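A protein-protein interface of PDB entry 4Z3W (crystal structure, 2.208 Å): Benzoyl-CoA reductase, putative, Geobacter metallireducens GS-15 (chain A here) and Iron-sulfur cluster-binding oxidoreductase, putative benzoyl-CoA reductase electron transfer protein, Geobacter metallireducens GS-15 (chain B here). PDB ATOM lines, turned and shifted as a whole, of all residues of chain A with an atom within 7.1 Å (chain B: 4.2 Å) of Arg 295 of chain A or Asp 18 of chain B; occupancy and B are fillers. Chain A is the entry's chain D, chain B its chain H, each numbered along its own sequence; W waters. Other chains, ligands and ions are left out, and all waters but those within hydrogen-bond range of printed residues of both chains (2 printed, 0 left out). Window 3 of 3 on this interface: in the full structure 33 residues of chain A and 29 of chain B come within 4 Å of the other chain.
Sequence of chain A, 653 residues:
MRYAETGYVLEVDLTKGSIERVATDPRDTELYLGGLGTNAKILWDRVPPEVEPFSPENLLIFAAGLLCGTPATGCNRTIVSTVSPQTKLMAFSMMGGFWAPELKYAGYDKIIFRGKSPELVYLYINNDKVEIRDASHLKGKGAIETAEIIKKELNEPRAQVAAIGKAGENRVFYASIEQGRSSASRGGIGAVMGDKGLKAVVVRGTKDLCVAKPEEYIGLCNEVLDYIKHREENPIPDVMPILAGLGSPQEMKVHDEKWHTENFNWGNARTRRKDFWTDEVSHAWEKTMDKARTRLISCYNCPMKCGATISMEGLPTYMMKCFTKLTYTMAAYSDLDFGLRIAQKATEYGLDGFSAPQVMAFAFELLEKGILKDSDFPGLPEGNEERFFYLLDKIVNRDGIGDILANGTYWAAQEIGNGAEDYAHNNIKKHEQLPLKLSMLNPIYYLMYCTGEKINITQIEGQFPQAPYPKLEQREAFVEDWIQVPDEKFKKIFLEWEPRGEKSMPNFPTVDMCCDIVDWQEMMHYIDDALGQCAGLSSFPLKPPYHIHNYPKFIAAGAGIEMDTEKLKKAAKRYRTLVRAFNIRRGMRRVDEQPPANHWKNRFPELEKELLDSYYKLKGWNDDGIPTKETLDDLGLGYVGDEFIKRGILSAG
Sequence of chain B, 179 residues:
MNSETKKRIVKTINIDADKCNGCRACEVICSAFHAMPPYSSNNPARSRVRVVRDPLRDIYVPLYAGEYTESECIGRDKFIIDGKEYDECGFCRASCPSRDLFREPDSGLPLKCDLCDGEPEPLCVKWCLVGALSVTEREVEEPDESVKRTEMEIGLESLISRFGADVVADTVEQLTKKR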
ATOM      1  N   MET A 252     -15.219   3.421  14.924  1.00  0.00           N
ATOM      2  CA  MET A 252     -13.784   3.566  14.718  1.00  0.00           C
ATOM      3  C   MET A 252     -13.405   5.053  14.759  1.00  0.00           C
ATOM      4  O   MET A 252     -12.325   5.396  15.228  1.00  0.00           O
ATOM      5  CB  MET A 252     -13.335   2.917  13.404  1.00  0.00           C
ATOM      6  CG  MET A 252     -13.533   1.374  13.311  1.00  0.00           C
ATOM      7  SD  MET A 252     -13.342   0.406  14.836  1.00  0.00           S
ATOM      8  CE  MET A 252     -11.578   0.149  14.916  1.00  0.00           C
ATOM      9  N   ALA A 292      -4.007   2.558  18.211  1.00  0.00           N
ATOM     10  CA  ALA A 292      -4.344   1.319  17.526  1.00  0.00           C
ATOM     11  C   ALA A 292      -4.800   1.555  16.092  1.00  0.00           C
ATOM     12  O   ALA A 292      -4.448   0.798  15.192  1.00  0.00           O
ATOM     13  CB  ALA A 292      -5.427   0.567  18.306  1.00  0.00           C
ATOM     14  N   ARG A 293      -5.599   2.598  15.890  1.00  0.00           N
ATOM     15  CA  ARG A 293      -6.212   2.861  14.591  1.00  0.00           C
ATOM     16  C   ARG A 293      -5.160   3.356  13.586  1.00  0.00           C
ATOM     17  O   ARG A 293      -4.660   4.468  13.690  1.00  0.00           O
ATOM     18  CB  ARG A 293      -7.349   3.883  14.747  1.00  0.00           C
ATOM     19  CG  ARG A 293      -8.265   4.024  13.540  1.00  0.00           C
ATOM     20  CD  ARG A 293      -9.351   5.094  13.765  1.00  0.00           C
ATOM     21  NE  ARG A 293      -8.775   6.357  14.214  1.00  0.00           N
ATOM     22  CZ  ARG A 293      -9.063   6.947  15.370  1.00  0.00           C
ATOM     23  NH1 ARG A 293      -9.953   6.413  16.197  1.00  0.00           N
ATOM     24  NH2 ARG A 293      -8.469   8.085  15.696  1.00  0.00           N
ATOM     25  N   THR A 294      -4.824   2.523  12.615  1.00  0.00           N
ATOM     26  CA  THR A 294      -3.819   2.886  11.631  1.00  0.00           C
ATOM     27  C   THR A 294      -4.425   3.798  10.561  1.00  0.00           C
ATOM     28  O   THR A 294      -3.882   4.859  10.245  1.00  0.00           O
ATOM     29  CB  THR A 294      -3.205   1.628  10.975  1.00  0.00           C
ATOM     30  OG1 THR A 294      -2.646   0.784  11.992  1.00  0.00           O
ATOM     31  CG2 THR A 294      -2.113   2.011   9.981  1.00  0.00           C
ATOM     32  N   ARG A 295      -5.560   3.384  10.013  1.00  0.00           N
ATOM     33  CA  ARG A 295      -6.281   4.180   9.031  1.00  0.00           C
ATOM     34  C   ARG A 295      -7.767   3.814   9.032  1.00  0.00           C
ATOM     35  O   ARG A 295      -8.124   2.649   9.234  1.00  0.00           O
ATOM     36  CB  ARG A 295      -5.695   3.974   7.628  1.00  0.00           C
ATOM     37  CG  ARG A 295      -6.248   4.926   6.560  1.00  0.00           C
ATOM     38  CD  ARG A 295      -5.574   4.709   5.216  1.00  0.00           C
ATOM     39  NE  ARG A 295      -4.129   4.905   5.301  1.00  0.00           N
ATOM     40  CZ  ARG A 295      -3.429   5.676   4.472  1.00  0.00           C
ATOM     41  NH1 ARG A 295      -4.037   6.319   3.486  1.00  0.00           N
ATOM     42  NH2 ARG A 295      -2.121   5.804   4.628  1.00  0.00           N
ATOM     43  N   LEU A 296      -8.615   4.818   8.806  1.00  0.00           N
ATOM     44  CA  LEU A 296     -10.009   4.614   8.459  1.00  0.00           C
ATOM     45  C   LEU A 296     -10.123   4.301   6.973  1.00  0.00           C
ATOM     46  O   LEU A 296      -9.634   5.063   6.134  1.00  0.00           O
ATOM     47  CB  LEU A 296     -10.833   5.854   8.811  1.00  0.00           C
ATOM     48  CG  LEU A 296     -10.875   6.183  10.300  1.00  0.00           C
ATOM     49  CD1 LEU A 296     -11.172   7.646  10.490  1.00  0.00           C
ATOM     50  CD2 LEU A 296     -11.923   5.317  10.992  1.00  0.00           C
ATOM     51  N   ILE A 297     -10.766   3.183   6.647  1.00  0.00           N
ATOM     52  CA  ILE A 297     -10.835   2.712   5.260  1.00  0.00           C
ATOM     53  C   ILE A 297     -12.267   2.351   4.837  1.00  0.00           C
ATOM     54  O   ILE A 297     -13.110   2.003   5.673  1.00  0.00           O
ATOM     55  CB  ILE A 297      -9.905   1.499   5.042  1.00  0.00           C
ATOM     56  CG1 ILE A 297     -10.184   0.393   6.060  1.00  0.00           C
ATOM     57  CG2 ILE A 297      -8.436   1.911   5.135  1.00  0.00           C
ATOM     58  CD1 ILE A 297      -9.555  -0.968   5.654  1.00  0.00           C
ATOM     59  N   LYS A 305     -15.928   5.534   4.837  1.00  0.00           N
ATOM     60  CA  LYS A 305     -14.767   4.908   5.503  1.00  0.00           C
ATOM     61  C   LYS A 305     -15.012   4.530   6.971  1.00  0.00           C
ATOM     62  O   LYS A 305     -14.366   5.055   7.887  1.00  0.00           O
ATOM     63  CB  LYS A 305     -13.536   5.820   5.391  1.00  0.00           C
ATOM     64  CG  LYS A 305     -13.660   7.200   6.032  1.00  0.00           C
ATOM     65  CD  LYS A 305     -12.469   8.102   5.613  1.00  0.00           C
ATOM     66  CE  LYS A 305     -12.630   9.536   6.141  1.00  0.00           C
ATOM     67  NZ  LYS A 305     -11.464  10.409   5.839  1.00  0.00           N
ATOM     68  N   GLY A 307     -14.661   1.508   8.520  1.00  0.00           N
ATOM     69  CA  GLY A 307     -13.774   0.533   9.120  1.00  0.00           C
ATOM     70  C   GLY A 307     -12.397   1.115   9.354  1.00  0.00           C
ATOM     71  O   GLY A 307     -12.081   2.208   8.889  1.00  0.00           O
ATOM     72  N   ALA A 308     -11.571   0.381  10.086  1.00  0.00           N
ATOM     73  CA  ALA A 308     -10.213   0.812  10.349  1.00  0.00           C
ATOM     74  C   ALA A 308      -9.292  -0.397  10.399  1.00  0.00           C
ATOM     75  O   ALA A 308      -9.689  -1.466  10.863  1.00  0.00           O
ATOM     76  CB  ALA A 308     -10.144   1.594  11.648  1.00  0.00           C
ATOM     77  N   THR A 309      -8.075  -0.232   9.893  1.00  0.00           N
ATOM     78  CA  THR A 309      -7.020  -1.202  10.127  1.00  0.00           C
ATOM     79  C   THR A 309      -6.582  -1.019  11.573  1.00  0.00           C
ATOM     80  O   THR A 309      -6.454   0.116  12.040  1.00  0.00           O
ATOM     81  CB  THR A 309      -5.797  -0.997   9.184  1.00  0.00           C
ATOM     82  OG1 THR A 309      -5.528   0.404   9.049  1.00  0.00           O
ATOM     83  CG2 THR A 309      -6.045  -1.583   7.807  1.00  0.00           C
ATOM     84  N   ILE A 310      -6.333  -2.116  12.278  1.00  0.00           N
ATOM     85  CA  ILE A 310      -5.956  -2.053  13.689  1.00  0.00           C
ATOM     86  C   ILE A 310      -4.624  -2.755  13.939  1.00  0.00           C
ATOM     87  O   ILE A 310      -4.453  -3.929  13.591  1.00  0.00           O
ATOM     88  CB  ILE A 310      -7.021  -2.696  14.599  1.00  0.00           C
ATOM     89  CG1 ILE A 310      -8.401  -2.087  14.347  1.00  0.00           C
ATOM     90  CG2 ILE A 310      -6.614  -2.551  16.058  1.00  0.00           C
ATOM     91  CD1 ILE A 310      -8.603  -0.757  15.048  1.00  0.00           C
ATOM     92  N   MET A 319      -8.581  -5.812  10.458  1.00  0.00           N
ATOM     93  CA  MET A 319      -9.523  -4.733  10.205  1.00  0.00           C
ATOM     94  C   MET A 319     -10.795  -4.894  11.039  1.00  0.00           C
ATOM     95  O   MET A 319     -11.205  -6.014  11.338  1.00  0.00           O
ATOM     96  CB  MET A 319      -9.861  -4.668   8.717  1.00  0.00           C
ATOM     97  CG  MET A 319      -8.773  -3.992   7.879  1.00  0.00           C
ATOM     98  SD  MET A 319      -8.169  -5.036   6.537  1.00  0.00           S
ATOM     99  CE  MET A 319      -7.489  -6.389   7.495  1.00  0.00           C
ATOM    100  N   MET A 320     -11.412  -3.770  11.397  1.00  0.00           N
ATOM    101  CA  MET A 320     -12.571  -3.757  12.293  1.00  0.00           C
ATOM    102  C   MET A 320     -13.574  -2.675  11.923  1.00  0.00           C
ATOM    103  O   MET A 320     -13.217  -1.677  11.296  1.00  0.00           O
ATOM    104  CB  MET A 320     -12.116  -3.555  13.738  1.00  0.00           C
ATOM    105  CG  MET A 320     -13.254  -3.303  14.726  1.00  0.00           C
ATOM    106  SD  MET A 320     -12.679  -3.197  16.435  1.00  0.00           S
ATOM    107  CE  MET A 320     -12.485  -4.922  16.864  1.00  0.00           C
ATOM    108  N   ASP B  16      -2.927  13.380  -2.432  1.00  0.00           N
ATOM    109  CA  ASP B  16      -2.595  13.256  -1.019  1.00  0.00           C
ATOM    110  C   ASP B  16      -2.940  11.846  -0.545  1.00  0.00           C
ATOM    111  O   ASP B  16      -4.012  11.594  -0.005  1.00  0.00           O
ATOM    112  CB  ASP B  16      -3.325  14.319  -0.188  1.00  0.00           C
ATOM    113  CG  ASP B  16      -2.952  14.278   1.294  1.00  0.00           C
ATOM    114  OD1 ASP B  16      -2.456  13.239   1.795  1.00  0.00           O
ATOM    115  OD2 ASP B  16      -3.182  15.298   1.982  1.00  0.00           O
ATOM    116  N   ALA B  17      -1.996  10.939  -0.735  1.00  0.00           N
ATOM    117  CA  ALA B  17      -2.189   9.530  -0.436  1.00  0.00           C
ATOM    118  C   ALA B  17      -2.449   9.276   1.044  1.00  0.00           C
ATOM    119  O   ALA B  17      -2.886   8.185   1.439  1.00  0.00           O
ATOM    120  CB  ALA B  17      -0.980   8.747  -0.895  1.00  0.00           C
ATOM    121  N   ASP B  18      -2.167  10.272   1.870  1.00  0.00           N
ATOM    122  CA  ASP B  18      -2.465  10.145   3.286  1.00  0.00           C
ATOM    123  C   ASP B  18      -3.974  10.248   3.539  1.00  0.00           C
ATOM    124  O   ASP B  18      -4.446   9.868   4.589  1.00  0.00           O
ATOM    125  CB  ASP B  18      -1.732  11.215   4.088  1.00  0.00           C
ATOM    126  CG  ASP B  18      -0.276  10.900   4.268  1.00  0.00           C
ATOM    127  OD1 ASP B  18       0.080   9.694   4.225  1.00  0.00           O
ATOM    128  OD2 ASP B  18       0.499  11.860   4.458  1.00  0.00           O
ATOM    129  N   LYS B  19      -4.709  10.786   2.575  1.00  0.00           N
ATOM    130  CA  LYS B  19      -6.139  10.993   2.723  1.00  0.00           C
ATOM    131  C   LYS B  19      -6.924   9.911   2.003  1.00  0.00           C
ATOM    132  O   LYS B  19      -8.138   9.884   2.089  1.00  0.00           O
ATOM    133  CB  LYS B  19      -6.539  12.373   2.179  1.00  0.00           C
ATOM    134  CG  LYS B  19      -6.071  13.524   3.046  1.00  0.00           C
ATOM    135  CD  LYS B  19      -6.630  14.839   2.562  1.00  0.00           C
ATOM    136  CE  LYS B  19      -6.279  15.960   3.524  1.00  0.00           C
ATOM    137  NZ  LYS B  19      -6.640  17.280   2.948  1.00  0.00           N
ATOM    138  N   CYS B  20      -6.235   9.043   1.264  1.00  0.00           N
ATOM    139  CA  CYS B  20      -6.914   8.011   0.484  1.00  0.00           C
ATOM    140  C   CYS B  20      -7.451   6.890   1.377  1.00  0.00           C
ATOM    141  O   CYS B  20      -6.756   6.390   2.264  1.00  0.00           O
ATOM    142  CB  CYS B  20      -5.983   7.428  -0.581  1.00  0.00           C
ATOM    143  SG  CYS B  20      -6.779   6.188  -1.634  1.00  0.00           S
ATOM    144  N   ASP B  58      -0.627  -0.726   4.876  1.00  0.00           N
ATOM    145  CA  ASP B  58      -1.094   0.661   4.936  1.00  0.00           C
ATOM    146  C   ASP B  58      -0.654   1.416   3.685  1.00  0.00           C
ATOM    147  O   ASP B  58      -0.160   2.547   3.758  1.00  0.00           O
ATOM    148  CB  ASP B  58      -0.587   1.368   6.198  1.00  0.00           C
ATOM    149  CG  ASP B  58      -1.178   2.767   6.362  1.00  0.00           C
ATOM    150  OD1 ASP B  58      -2.418   2.916   6.320  1.00  0.00           O
ATOM    151  OD2 ASP B  58      -0.399   3.728   6.482  1.00  0.00           O
ATOM    152  N   TYR B  60      -1.928   3.047   0.207  1.00  0.00           N
ATOM    153  CA  TYR B  60      -3.040   3.476  -0.624  1.00  0.00           C
ATOM    154  C   TYR B  60      -2.533   4.620  -1.480  1.00  0.00           C
ATOM    155  O   TYR B  60      -2.454   5.759  -1.020  1.00  0.00           O
ATOM    156  CB  TYR B  60      -4.242   3.910   0.215  1.00  0.00           C
ATOM    157  CG  TYR B  60      -4.594   2.950   1.324  1.00  0.00           C
ATOM    158  CD1 TYR B  60      -3.822   2.888   2.474  1.00  0.00           C
ATOM    159  CD2 TYR B  60      -5.713   2.117   1.231  1.00  0.00           C
ATOM    160  CE1 TYR B  60      -4.128   2.010   3.495  1.00  0.00           C
ATOM    161  CE2 TYR B  60      -6.045   1.234   2.264  1.00  0.00           C
ATOM    162  CZ  TYR B  60      -5.242   1.190   3.390  1.00  0.00           C
ATOM    163  OH  TYR B  60      -5.531   0.325   4.418  1.00  0.00           O
HETATM  164  O   HOH W   1       0.077   7.038   3.090  1.00  0.00           O
HETATM  165  O   HOH W   2      -4.009   0.412   6.812  1.00  0.00           O
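Hydrophobic or aromatic side chains of chain A that line the printed part of chain B: Ile 297.
Among the printed residues, Asp or Glu carboxylates within 4 Å of a Lys or Arg side-chain nitrogen of the other chain: Arg 295 of chain A with Asp 58 of chain B (2.8 Å).
The backbone NH (N) of Ile 297 of chain A lies within hydrogen-bond range of the backbone carbonyl oxygen (O) of Gly 307 of chain A, at 2.8 Å.
The backbone carbonyl oxygen of Arg 295 of chain A lies within hydrogen-bond range of the backbone NH of Thr 309 of chain A (3.0 Å).
OD1 of Asp 16 of chain B sits at hydrogen-bond distance from N of Asp 18 of chain B, 3.0 Å away.
The backbone carbonyl oxygen (O) of Thr 309 of chain A lies within hydrogen-bond range of the backbone NH (N) of Thr 294 of chain A, at 3.0 Å.
NH1 of Arg 295 of chain A is in hydrogen-bond range of O of Cys 20 of chain B.
The guanidinium group of Arg 295 of chain A is in salt-bridge range of the side-chain carboxylate of Asp 58 of chain B.
The guanidinium group of Arg 295 of chain A lies within hydrogen-bond range of the backbone carbonyl oxygen of Ala 17 of chain B, 3.0 Å away.
Met 252 of chain A touches none of the printed residues of chain B.
Printed residues of chain B within 4 Å of Thr 294 of chain A: Asp 58 (3.8 Å).
Of chain B, only Ala 17 (3.0 Å), Asp 18 (3.7 Å), Cys 20 (3.0 Å), Asp 58 (2.8 Å) and Tyr 60 (3.4 Å) come within 4 Å of Arg 295 of chain A.
Asp 18 of chain B touches just one residue of chain A: Arg 295.
Printed residues of chain A within 4 Å of Asp 58 of chain B: Thr 294 (3.8 Å) and Arg 295 (2.8 Å).
Of the printed residues of chain A, Tyr 60 of chain B touches Arg 295, Ile 297 and Thr 309.
The nearest printed residue of chain B that does not touch Arg 295 of chain A is Lys 19 of chain B (4.6 Å).
Thr 294 of chain A touches Asp 58 of chain B.
NH1 of Arg 295 of chain A touches O of Asp 18 of chain B (3.7 Å).
Arg 295 of chain A touches Tyr 60 of chain B (NE to CE1, 3.4 Å).
Ile 297 of chain A touches Tyr 60 of chain B (CG2 to OH, 3.4 Å).
CG2 of Thr 309 of chain A touches OH of Tyr 60 of chain B, at 3.9 Å.
Water W2 lies within hydrogen-bond range of OG1 of Thr 309 of chain A, OH of Tyr 60 of chain B and OD1 of Asp 58 of chain B.
Water W1 bridges OD1 of Asp 18 of chain B (2.9 Å) and NH2 of Arg 295 of chain A (3.0 Å).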
